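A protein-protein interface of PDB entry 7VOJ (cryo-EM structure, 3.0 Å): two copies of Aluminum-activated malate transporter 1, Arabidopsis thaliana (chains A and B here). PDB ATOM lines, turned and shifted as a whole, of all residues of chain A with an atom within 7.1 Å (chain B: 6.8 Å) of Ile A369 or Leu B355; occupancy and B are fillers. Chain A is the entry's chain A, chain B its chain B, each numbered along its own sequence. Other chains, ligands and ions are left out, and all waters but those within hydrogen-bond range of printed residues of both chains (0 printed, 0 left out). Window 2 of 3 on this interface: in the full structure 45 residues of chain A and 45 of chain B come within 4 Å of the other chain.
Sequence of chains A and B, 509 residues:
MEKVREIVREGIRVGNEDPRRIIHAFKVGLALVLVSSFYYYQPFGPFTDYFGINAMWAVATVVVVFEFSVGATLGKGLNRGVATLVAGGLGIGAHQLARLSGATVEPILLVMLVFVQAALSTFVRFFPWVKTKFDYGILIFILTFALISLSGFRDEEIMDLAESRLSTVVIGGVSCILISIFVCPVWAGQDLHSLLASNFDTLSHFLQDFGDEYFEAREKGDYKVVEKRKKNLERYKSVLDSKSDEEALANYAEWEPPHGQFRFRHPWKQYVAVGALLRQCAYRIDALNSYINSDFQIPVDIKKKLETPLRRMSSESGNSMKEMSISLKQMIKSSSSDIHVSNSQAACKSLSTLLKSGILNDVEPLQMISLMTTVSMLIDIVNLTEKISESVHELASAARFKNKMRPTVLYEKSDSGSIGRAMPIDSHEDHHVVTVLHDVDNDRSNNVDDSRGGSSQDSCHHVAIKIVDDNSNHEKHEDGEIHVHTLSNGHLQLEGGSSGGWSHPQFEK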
ATOM      1  N   TYR A 291     -12.613  -8.484 -20.332  1.00  0.00           N
ATOM      2  CA  TYR A 291     -13.616  -8.405 -19.276  1.00  0.00           C
ATOM      3  C   TYR A 291     -14.977  -8.044 -19.850  1.00  0.00           C
ATOM      4  O   TYR A 291     -16.002  -8.577 -19.428  1.00  0.00           O
ATOM      5  CB  TYR A 291     -13.201  -7.428 -18.177  1.00  0.00           C
ATOM      6  CG  TYR A 291     -12.710  -8.124 -16.930  1.00  0.00           C
ATOM      7  CD1 TYR A 291     -11.387  -8.522 -16.805  1.00  0.00           C
ATOM      8  CD2 TYR A 291     -13.579  -8.401 -15.883  1.00  0.00           C
ATOM      9  CE1 TYR A 291     -10.940  -9.166 -15.668  1.00  0.00           C
ATOM     10  CE2 TYR A 291     -13.141  -9.044 -14.742  1.00  0.00           C
ATOM     11  CZ  TYR A 291     -11.821  -9.424 -14.640  1.00  0.00           C
ATOM     12  OH  TYR A 291     -11.380 -10.066 -13.505  1.00  0.00           O
ATOM     13  N   PHE A 296     -19.301 -13.914 -17.274  1.00  0.00           N
ATOM     14  CA  PHE A 296     -19.559 -13.446 -15.917  1.00  0.00           C
ATOM     15  C   PHE A 296     -19.643 -11.929 -15.951  1.00  0.00           C
ATOM     16  O   PHE A 296     -18.625 -11.234 -15.982  1.00  0.00           O
ATOM     17  CB  PHE A 296     -18.468 -13.925 -14.965  1.00  0.00           C
ATOM     18  CG  PHE A 296     -18.476 -13.229 -13.628  1.00  0.00           C
ATOM     19  CD1 PHE A 296     -19.583 -13.301 -12.795  1.00  0.00           C
ATOM     20  CD2 PHE A 296     -17.372 -12.505 -13.207  1.00  0.00           C
ATOM     21  CE1 PHE A 296     -19.592 -12.657 -11.571  1.00  0.00           C
ATOM     22  CE2 PHE A 296     -17.372 -11.862 -11.980  1.00  0.00           C
ATOM     23  CZ  PHE A 296     -18.484 -11.938 -11.163  1.00  0.00           C
ATOM     24  N   ILE A 298     -21.396  -8.435 -14.155  1.00  0.00           N
ATOM     25  CA  ILE A 298     -22.038  -7.870 -12.964  1.00  0.00           C
ATOM     26  C   ILE A 298     -23.451  -7.433 -13.326  1.00  0.00           C
ATOM     27  O   ILE A 298     -23.706  -7.104 -14.499  1.00  0.00           O
ATOM     28  CB  ILE A 298     -21.213  -6.692 -12.445  1.00  0.00           C
ATOM     29  CG1 ILE A 298     -19.726  -6.999 -12.578  1.00  0.00           C
ATOM     30  CG2 ILE A 298     -21.524  -6.389 -10.997  1.00  0.00           C
ATOM     31  CD1 ILE A 298     -18.849  -5.846 -12.184  1.00  0.00           C
ATOM     32  N   GLU A 364     -21.446  -7.922  -3.392  1.00  0.00           N
ATOM     33  CA  GLU A 364     -20.664  -9.142  -3.275  1.00  0.00           C
ATOM     34  C   GLU A 364     -19.231  -8.888  -3.739  1.00  0.00           C
ATOM     35  O   GLU A 364     -19.012  -8.127  -4.689  1.00  0.00           O
ATOM     36  CB  GLU A 364     -21.297 -10.262  -4.104  1.00  0.00           C
ATOM     37  CG  GLU A 364     -22.489 -10.943  -3.444  1.00  0.00           C
ATOM     38  CD  GLU A 364     -23.740 -10.083  -3.433  1.00  0.00           C
ATOM     39  OE1 GLU A 364     -23.873  -9.218  -4.321  1.00  0.00           O
ATOM     40  OE2 GLU A 364     -24.583 -10.264  -2.530  1.00  0.00           O
ATOM     41  N   PRO A 365     -18.234  -9.497  -3.090  1.00  0.00           N
ATOM     42  CA  PRO A 365     -16.839  -9.116  -3.366  1.00  0.00           C
ATOM     43  C   PRO A 365     -16.293  -9.626  -4.690  1.00  0.00           C
ATOM     44  O   PRO A 365     -15.277  -9.097  -5.152  1.00  0.00           O
ATOM     45  CB  PRO A 365     -16.074  -9.712  -2.182  1.00  0.00           C
ATOM     46  CG  PRO A 365     -16.926 -10.836  -1.720  1.00  0.00           C
ATOM     47  CD  PRO A 365     -18.336 -10.402  -1.933  1.00  0.00           C
ATOM     48  N   LEU A 366     -16.912 -10.630  -5.313  1.00  0.00           N
ATOM     49  CA  LEU A 366     -16.463 -11.048  -6.639  1.00  0.00           C
ATOM     50  C   LEU A 366     -16.838 -10.008  -7.684  1.00  0.00           C
ATOM     51  O   LEU A 366     -16.066  -9.727  -8.618  1.00  0.00           O
ATOM     52  CB  LEU A 366     -17.058 -12.410  -6.998  1.00  0.00           C
ATOM     53  CG  LEU A 366     -16.673 -13.657  -6.190  1.00  0.00           C
ATOM     54  CD1 LEU A 366     -17.481 -14.871  -6.612  1.00  0.00           C
ATOM     55  CD2 LEU A 366     -15.182 -13.946  -6.255  1.00  0.00           C
ATOM     56  N   GLN A 367     -18.021  -9.416  -7.531  1.00  0.00           N
ATOM     57  CA  GLN A 367     -18.381  -8.247  -8.316  1.00  0.00           C
ATOM     58  C   GLN A 367     -17.447  -7.085  -8.026  1.00  0.00           C
ATOM     59  O   GLN A 367     -17.125  -6.307  -8.930  1.00  0.00           O
ATOM     60  CB  GLN A 367     -19.824  -7.866  -8.016  1.00  0.00           C
ATOM     61  CG  GLN A 367     -20.779  -9.034  -8.129  1.00  0.00           C
ATOM     62  CD  GLN A 367     -22.078  -8.785  -7.410  1.00  0.00           C
ATOM     63  OE1 GLN A 367     -22.139  -7.989  -6.475  1.00  0.00           O
ATOM     64  NE2 GLN A 367     -23.131  -9.463  -7.844  1.00  0.00           N
ATOM     65  N   MET A 368     -16.975  -6.974  -6.781  1.00  0.00           N
ATOM     66  CA  MET A 368     -15.973  -5.971  -6.454  1.00  0.00           C
ATOM     67  C   MET A 368     -14.639  -6.269  -7.116  1.00  0.00           C
ATOM     68  O   MET A 368     -13.882  -5.341  -7.405  1.00  0.00           O
ATOM     69  CB  MET A 368     -15.797  -5.874  -4.942  1.00  0.00           C
ATOM     70  CG  MET A 368     -16.888  -5.099  -4.249  1.00  0.00           C
ATOM     71  SD  MET A 368     -16.535  -3.339  -4.262  1.00  0.00           S
ATOM     72  CE  MET A 368     -15.036  -3.306  -3.286  1.00  0.00           C
ATOM     73  N   ILE A 369     -14.338  -7.543  -7.373  1.00  0.00           N
ATOM     74  CA  ILE A 369     -13.106  -7.886  -8.077  1.00  0.00           C
ATOM     75  C   ILE A 369     -13.159  -7.379  -9.510  1.00  0.00           C
ATOM     76  O   ILE A 369     -12.225  -6.720  -9.985  1.00  0.00           O
ATOM     77  CB  ILE A 369     -12.856  -9.404  -8.022  1.00  0.00           C
ATOM     78  CG1 ILE A 369     -12.390  -9.814  -6.629  1.00  0.00           C
ATOM     79  CG2 ILE A 369     -11.849  -9.836  -9.076  1.00  0.00           C
ATOM     80  CD1 ILE A 369     -12.056 -11.275  -6.509  1.00  0.00           C
ATOM     81  N   SER A 370     -14.274  -7.635 -10.201  1.00  0.00           N
ATOM     82  CA  SER A 370     -14.409  -7.145 -11.574  1.00  0.00           C
ATOM     83  C   SER A 370     -14.475  -5.621 -11.622  1.00  0.00           C
ATOM     84  O   SER A 370     -13.879  -4.992 -12.509  1.00  0.00           O
ATOM     85  CB  SER A 370     -15.644  -7.750 -12.230  1.00  0.00           C
ATOM     86  OG  SER A 370     -15.581  -9.164 -12.210  1.00  0.00           O
ATOM     87  N   LEU A 371     -15.141  -5.014 -10.638  1.00  0.00           N
ATOM     88  CA  LEU A 371     -15.292  -3.565 -10.616  1.00  0.00           C
ATOM     89  C   LEU A 371     -13.964  -2.873 -10.345  1.00  0.00           C
ATOM     90  O   LEU A 371     -13.606  -1.911 -11.036  1.00  0.00           O
ATOM     91  CB  LEU A 371     -16.327  -3.168  -9.568  1.00  0.00           C
ATOM     92  CG  LEU A 371     -17.240  -2.004  -9.928  1.00  0.00           C
ATOM     93  CD1 LEU A 371     -17.977  -2.318 -11.205  1.00  0.00           C
ATOM     94  CD2 LEU A 371     -18.218  -1.741  -8.805  1.00  0.00           C
ATOM     95  N   MET A 372     -13.206  -3.359  -9.362  1.00  0.00           N
ATOM     96  CA  MET A 372     -11.934  -2.730  -9.048  1.00  0.00           C
ATOM     97  C   MET A 372     -10.872  -3.024 -10.094  1.00  0.00           C
ATOM     98  O   MET A 372      -9.940  -2.227 -10.243  1.00  0.00           O
ATOM     99  CB  MET A 372     -11.448  -3.162  -7.671  1.00  0.00           C
ATOM    100  CG  MET A 372     -12.291  -2.646  -6.522  1.00  0.00           C
ATOM    101  SD  MET A 372     -12.872  -0.971  -6.788  1.00  0.00           S
ATOM    102  CE  MET A 372     -13.303  -0.504  -5.120  1.00  0.00           C
ATOM    103  N   THR A 373     -11.014  -4.118 -10.846  1.00  0.00           N
ATOM    104  CA  THR A 373     -10.163  -4.325 -12.012  1.00  0.00           C
ATOM    105  C   THR A 373     -10.399  -3.249 -13.060  1.00  0.00           C
ATOM    106  O   THR A 373      -9.445  -2.685 -13.610  1.00  0.00           O
ATOM    107  CB  THR A 373     -10.423  -5.693 -12.622  1.00  0.00           C
ATOM    108  OG1 THR A 373     -10.554  -6.661 -11.582  1.00  0.00           O
ATOM    109  CG2 THR A 373      -9.280  -6.075 -13.534  1.00  0.00           C
ATOM    110  N   THR A 374     -11.674  -2.953 -13.348  1.00  0.00           N
ATOM    111  CA  THR A 374     -11.992  -1.956 -14.366  1.00  0.00           C
ATOM    112  C   THR A 374     -11.576  -0.555 -13.936  1.00  0.00           C
ATOM    113  O   THR A 374     -11.083   0.231 -14.755  1.00  0.00           O
ATOM    114  CB  THR A 374     -13.480  -1.989 -14.680  1.00  0.00           C
ATOM    115  OG1 THR A 374     -14.214  -2.005 -13.454  1.00  0.00           O
ATOM    116  CG2 THR A 374     -13.822  -3.223 -15.477  1.00  0.00           C
ATOM    117  N   VAL A 375     -11.748  -0.235 -12.653  1.00  0.00           N
ATOM    118  CA  VAL A 375     -11.335   1.071 -12.148  1.00  0.00           C
ATOM    119  C   VAL A 375      -9.818   1.213 -12.199  1.00  0.00           C
ATOM    120  O   VAL A 375      -9.295   2.276 -12.563  1.00  0.00           O
ATOM    121  CB  VAL A 375     -11.892   1.283 -10.730  1.00  0.00           C
ATOM    122  CG1 VAL A 375     -11.361   2.554 -10.117  1.00  0.00           C
ATOM    123  CG2 VAL A 375     -13.392   1.351 -10.776  1.00  0.00           C
ATOM    124  N   SER A 376      -9.089   0.133 -11.899  1.00  0.00           N
ATOM    125  CA  SER A 376      -7.631   0.180 -11.961  1.00  0.00           C
ATOM    126  C   SER A 376      -7.135   0.345 -13.389  1.00  0.00           C
ATOM    127  O   SER A 376      -6.179   1.091 -13.635  1.00  0.00           O
ATOM    128  CB  SER A 376      -7.047  -1.083 -11.351  1.00  0.00           C
ATOM    129  OG  SER A 376      -7.757  -1.441 -10.185  1.00  0.00           O
ATOM    130  N   LEU B 306      -3.802 -11.887   2.971  1.00  0.00           N
ATOM    131  CA  LEU B 306      -4.061 -12.628   1.742  1.00  0.00           C
ATOM    132  C   LEU B 306      -2.843 -13.418   1.283  1.00  0.00           C
ATOM    133  O   LEU B 306      -2.856 -13.970   0.183  1.00  0.00           O
ATOM    134  CB  LEU B 306      -4.502 -11.686   0.623  1.00  0.00           C
ATOM    135  CG  LEU B 306      -5.974 -11.306   0.532  1.00  0.00           C
ATOM    136  CD1 LEU B 306      -6.217 -10.494  -0.718  1.00  0.00           C
ATOM    137  CD2 LEU B 306      -6.826 -12.543   0.522  1.00  0.00           C
ATOM    138  N   CYS B 348      -7.481 -21.248  -6.221  1.00  0.00           N
ATOM    139  CA  CYS B 348      -8.367 -20.153  -6.613  1.00  0.00           C
ATOM    140  C   CYS B 348      -9.743 -20.299  -5.979  1.00  0.00           C
ATOM    141  O   CYS B 348     -10.335 -19.307  -5.538  1.00  0.00           O
ATOM    142  CB  CYS B 348      -8.489 -20.083  -8.133  1.00  0.00           C
ATOM    143  SG  CYS B 348      -7.145 -19.203  -8.955  1.00  0.00           S
ATOM    144  N   SER B 350     -10.237 -21.820  -3.139  1.00  0.00           N
ATOM    145  CA  SER B 350     -10.014 -21.501  -1.733  1.00  0.00           C
ATOM    146  C   SER B 350      -9.968 -19.998  -1.501  1.00  0.00           C
ATOM    147  O   SER B 350     -10.430 -19.520  -0.459  1.00  0.00           O
ATOM    148  CB  SER B 350      -8.725 -22.147  -1.237  1.00  0.00           C
ATOM    149  OG  SER B 350      -8.857 -23.555  -1.175  1.00  0.00           O
ATOM    150  N   LEU B 351      -9.441 -19.237  -2.460  1.00  0.00           N
ATOM    151  CA  LEU B 351      -9.475 -17.784  -2.331  1.00  0.00           C
ATOM    152  C   LEU B 351     -10.894 -17.253  -2.476  1.00  0.00           C
ATOM    153  O   LEU B 351     -11.279 -16.299  -1.790  1.00  0.00           O
ATOM    154  CB  LEU B 351      -8.556 -17.138  -3.364  1.00  0.00           C
ATOM    155  CG  LEU B 351      -8.415 -15.620  -3.255  1.00  0.00           C
ATOM    156  CD1 LEU B 351      -7.946 -15.238  -1.871  1.00  0.00           C
ATOM    157  CD2 LEU B 351      -7.462 -15.098  -4.301  1.00  0.00           C
ATOM    158  N   SER B 352     -11.688 -17.872  -3.351  1.00  0.00           N
ATOM    159  CA  SER B 352     -13.072 -17.447  -3.533  1.00  0.00           C
ATOM    160  C   SER B 352     -13.909 -17.720  -2.290  1.00  0.00           C
ATOM    161  O   SER B 352     -14.841 -16.965  -1.991  1.00  0.00           O
ATOM    162  CB  SER B 352     -13.679 -18.144  -4.747  1.00  0.00           C
ATOM    163  OG  SER B 352     -15.086 -17.998  -4.762  1.00  0.00           O
ATOM    164  N   THR B 353     -13.600 -18.789  -1.552  1.00  0.00           N
ATOM    165  CA  THR B 353     -14.283 -18.994  -0.278  1.00  0.00           C
ATOM    166  C   THR B 353     -13.678 -18.141   0.827  1.00  0.00           C
ATOM    167  O   THR B 353     -14.339 -17.886   1.838  1.00  0.00           O
ATOM    168  CB  THR B 353     -14.258 -20.466   0.129  1.00  0.00           C
ATOM    169  OG1 THR B 353     -12.906 -20.891   0.319  1.00  0.00           O
ATOM    170  CG2 THR B 353     -14.911 -21.320  -0.935  1.00  0.00           C
ATOM    171  N   LEU B 354     -12.430 -17.698   0.663  1.00  0.00           N
ATOM    172  CA  LEU B 354     -11.840 -16.811   1.659  1.00  0.00           C
ATOM    173  C   LEU B 354     -12.393 -15.398   1.547  1.00  0.00           C
ATOM    174  O   LEU B 354     -12.480 -14.689   2.554  1.00  0.00           O
ATOM    175  CB  LEU B 354     -10.319 -16.796   1.514  1.00  0.00           C
ATOM    176  CG  LEU B 354      -9.479 -16.242   2.670  1.00  0.00           C
ATOM    177  CD1 LEU B 354      -8.240 -17.085   2.839  1.00  0.00           C
ATOM    178  CD2 LEU B 354      -9.077 -14.801   2.448  1.00  0.00           C
ATOM    179  N   LEU B 355     -12.758 -14.969   0.338  1.00  0.00           N
ATOM    180  CA  LEU B 355     -13.204 -13.595   0.148  1.00  0.00           C
ATOM    181  C   LEU B 355     -14.612 -13.372   0.678  1.00  0.00           C
ATOM    182  O   LEU B 355     -14.954 -12.249   1.062  1.00  0.00           O
ATOM    183  CB  LEU B 355     -13.122 -13.225  -1.327  1.00  0.00           C
ATOM    184  CG  LEU B 355     -11.694 -12.944  -1.778  1.00  0.00           C
ATOM    185  CD1 LEU B 355     -11.521 -13.268  -3.240  1.00  0.00           C
ATOM    186  CD2 LEU B 355     -11.357 -11.499  -1.522  1.00  0.00           C
ATOM    187  N   LYS B 356     -15.435 -14.420   0.722  1.00  0.00           N
ATOM    188  CA  LYS B 356     -16.759 -14.306   1.319  1.00  0.00           C
ATOM    189  C   LYS B 356     -16.712 -14.212   2.836  1.00  0.00           C
ATOM    190  O   LYS B 356     -17.712 -13.817   3.445  1.00  0.00           O
ATOM    191  CB  LYS B 356     -17.625 -15.496   0.916  1.00  0.00           C
ATOM    192  CG  LYS B 356     -17.820 -15.652  -0.572  1.00  0.00           C
ATOM    193  CD  LYS B 356     -18.644 -16.889  -0.871  1.00  0.00           C
ATOM    194  CE  LYS B 356     -18.626 -17.215  -2.349  1.00  0.00           C
ATOM    195  NZ  LYS B 356     -19.102 -16.065  -3.152  1.00  0.00           N
ATOM    196  N   SER B 357     -15.581 -14.552   3.456  1.00  0.00           N
ATOM    197  CA  SER B 357     -15.461 -14.497   4.907  1.00  0.00           C
ATOM    198  C   SER B 357     -15.378 -13.071   5.435  1.00  0.00           C
ATOM    199  O   SER B 357     -15.482 -12.870   6.650  1.00  0.00           O
ATOM    200  CB  SER B 357     -14.238 -15.289   5.358  1.00  0.00           C
ATOM    201  OG  SER B 357     -14.037 -15.164   6.753  1.00  0.00           O
ATOM    202  N   GLY B 358     -15.184 -12.088   4.564  1.00  0.00           N
ATOM    203  CA  GLY B 358     -15.209 -10.700   4.981  1.00  0.00           C
ATOM    204  C   GLY B 358     -13.981 -10.264   5.743  1.00  0.00           C
ATOM    205  O   GLY B 358     -14.091  -9.491   6.703  1.00  0.00           O
ATOM    206  N   ILE B 359     -12.805 -10.741   5.342  1.00  0.00           N
ATOM    207  CA  ILE B 359     -11.583 -10.320   6.011  1.00  0.00           C
ATOM    208  C   ILE B 359     -11.119  -8.961   5.504  1.00  0.00           C
ATOM    209  O   ILE B 359     -10.242  -8.339   6.118  1.00  0.00           O
ATOM    210  CB  ILE B 359     -10.508 -11.408   5.848  1.00  0.00           C
ATOM    211  CG1 ILE B 359      -9.527 -11.396   7.021  1.00  0.00           C
ATOM    212  CG2 ILE B 359      -9.769 -11.255   4.538  1.00  0.00           C
ATOM    213  CD1 ILE B 359      -8.478 -12.483   6.937  1.00  0.00           C
ATOM    214  N   LEU B 360     -11.712  -8.465   4.414  1.00  0.00           N
ATOM    215  CA  LEU B 360     -11.384  -7.160   3.856  1.00  0.00           C
ATOM    216  C   LEU B 360     -12.442  -6.105   4.156  1.00  0.00           C
ATOM    217  O   LEU B 360     -12.784  -5.311   3.271  1.00  0.00           O
ATOM    218  CB  LEU B 360     -11.165  -7.264   2.347  1.00  0.00           C
ATOM    219  CG  LEU B 360      -9.991  -8.080   1.796  1.00  0.00           C
ATOM    220  CD1 LEU B 360     -10.011  -8.194   0.277  1.00  0.00           C
ATOM    221  CD2 LEU B 360      -8.680  -7.512   2.278  1.00  0.00           C
ATOM    222  N   MET B 372      -7.152  -5.715  -5.127  1.00  0.00           N
ATOM    223  CA  MET B 372      -8.010  -6.411  -6.072  1.00  0.00           C
ATOM    224  C   MET B 372      -7.453  -6.381  -7.485  1.00  0.00           C
ATOM    225  O   MET B 372      -7.769  -7.278  -8.274  1.00  0.00           O
ATOM    226  CB  MET B 372      -9.416  -5.829  -6.049  1.00  0.00           C
ATOM    227  CG  MET B 372     -10.176  -6.085  -4.762  1.00  0.00           C
ATOM    228  SD  MET B 372      -9.864  -7.716  -4.087  1.00  0.00           S
ATOM    229  CE  MET B 372     -11.257  -7.886  -2.984  1.00  0.00           C
ATOM    230  N   THR B 373      -6.605  -5.401  -7.807  1.00  0.00           N
ATOM    231  CA  THR B 373      -5.863  -5.453  -9.062  1.00  0.00           C
ATOM    232  C   THR B 373      -4.919  -6.644  -9.091  1.00  0.00           C
ATOM    233  O   THR B 373      -4.855  -7.375 -10.088  1.00  0.00           O
ATOM    234  CB  THR B 373      -5.070  -4.173  -9.263  1.00  0.00           C
ATOM    235  OG1 THR B 373      -5.870  -3.052  -8.886  1.00  0.00           O
ATOM    236  CG2 THR B 373      -4.659  -4.043 -10.712  1.00  0.00           C
ATOM    237  N   VAL B 375      -5.043  -9.419  -7.259  1.00  0.00           N
ATOM    238  CA  VAL B 375      -5.796 -10.670  -7.247  1.00  0.00           C
ATOM    239  C   VAL B 375      -6.371 -10.965  -8.627  1.00  0.00           C
ATOM    240  O   VAL B 375      -6.352 -12.116  -9.087  1.00  0.00           O
ATOM    241  CB  VAL B 375      -6.886 -10.614  -6.163  1.00  0.00           C
ATOM    242  CG1 VAL B 375      -7.780 -11.826  -6.222  1.00  0.00           C
ATOM    243  CG2 VAL B 375      -6.249 -10.542  -4.803  1.00  0.00           C
ATOM    244  N   SER B 376      -6.831  -9.929  -9.337  1.00  0.00           N
ATOM    245  CA  SER B 376      -7.363 -10.127 -10.681  1.00  0.00           C
ATOM    246  C   SER B 376      -6.277 -10.549 -11.658  1.00  0.00           C
ATOM    247  O   SER B 376      -6.508 -11.413 -12.513  1.00  0.00           O
ATOM    248  CB  SER B 376      -8.030  -8.850 -11.166  1.00  0.00           C
ATOM    249  OG  SER B 376      -8.773  -8.255 -10.124  1.00  0.00           O
ATOM    250  N   ILE B 379      -5.449 -14.292 -10.977  1.00  0.00           N
ATOM    251  CA  ILE B 379      -6.492 -15.193 -11.468  1.00  0.00           C
ATOM    252  C   ILE B 379      -6.440 -15.290 -12.988  1.00  0.00           C
ATOM    253  O   ILE B 379      -6.612 -16.376 -13.567  1.00  0.00           O
ATOM    254  CB  ILE B 379      -7.868 -14.730 -10.959  1.00  0.00           C
ATOM    255  CG1 ILE B 379      -7.951 -14.917  -9.452  1.00  0.00           C
ATOM    256  CG2 ILE B 379      -8.993 -15.511 -11.597  1.00  0.00           C
ATOM    257  CD1 ILE B 379      -9.244 -14.458  -8.857  1.00  0.00           C
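OG1 of Thr A373 sits at hydrogen-bond distance from OG of Ser B376 (2.8 Å).
The side-chain hydroxyl of Thr B373 sits at hydrogen-bond distance from the side-chain hydroxyl of Ser A376.
Among the printed residues, pairs that only touch across the chains: Pro A365 with Leu B355 (3.7 Å), Ile A369 with Leu B355 (3.9 Å), Ile A369 with Ser B376 (3.6 Å) and Met A372 with Met B372 (3.7 Å).
Ile A369 touches two residues of chain B.
Of the printed residues of chain B, Met A372 touches Met B372 (3.7 Å).
Printed residues of chain B within 4 Å of Thr A373: Ser B376 (2.8 Å).
Of the printed residues of chain B, Ser A376 touches Thr B373.
Leu B355 touches two residues of chain A.
Printed residues of chain A within 4 Å of Met B372: Met A372.
Printed residues of chain A within 4 Å of Thr B373: Ser A376.
Val B375 touches none of the printed residues of chain A.
The nearest printed residue of chain B that does not touch Pro A365 is Lys B356 (4.6 Å).
Along chain B the printed residues that touch a printed residue of chain A span positions 355 to 376.
Of the 16 printed residues of chain A, 5 touch a printed residue of chain B.
Met A372 touches its own counterpart, Met B372.
Thr A373 touches Ser B376, and with the chains exchanged Ser A376 touches Thr B373.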
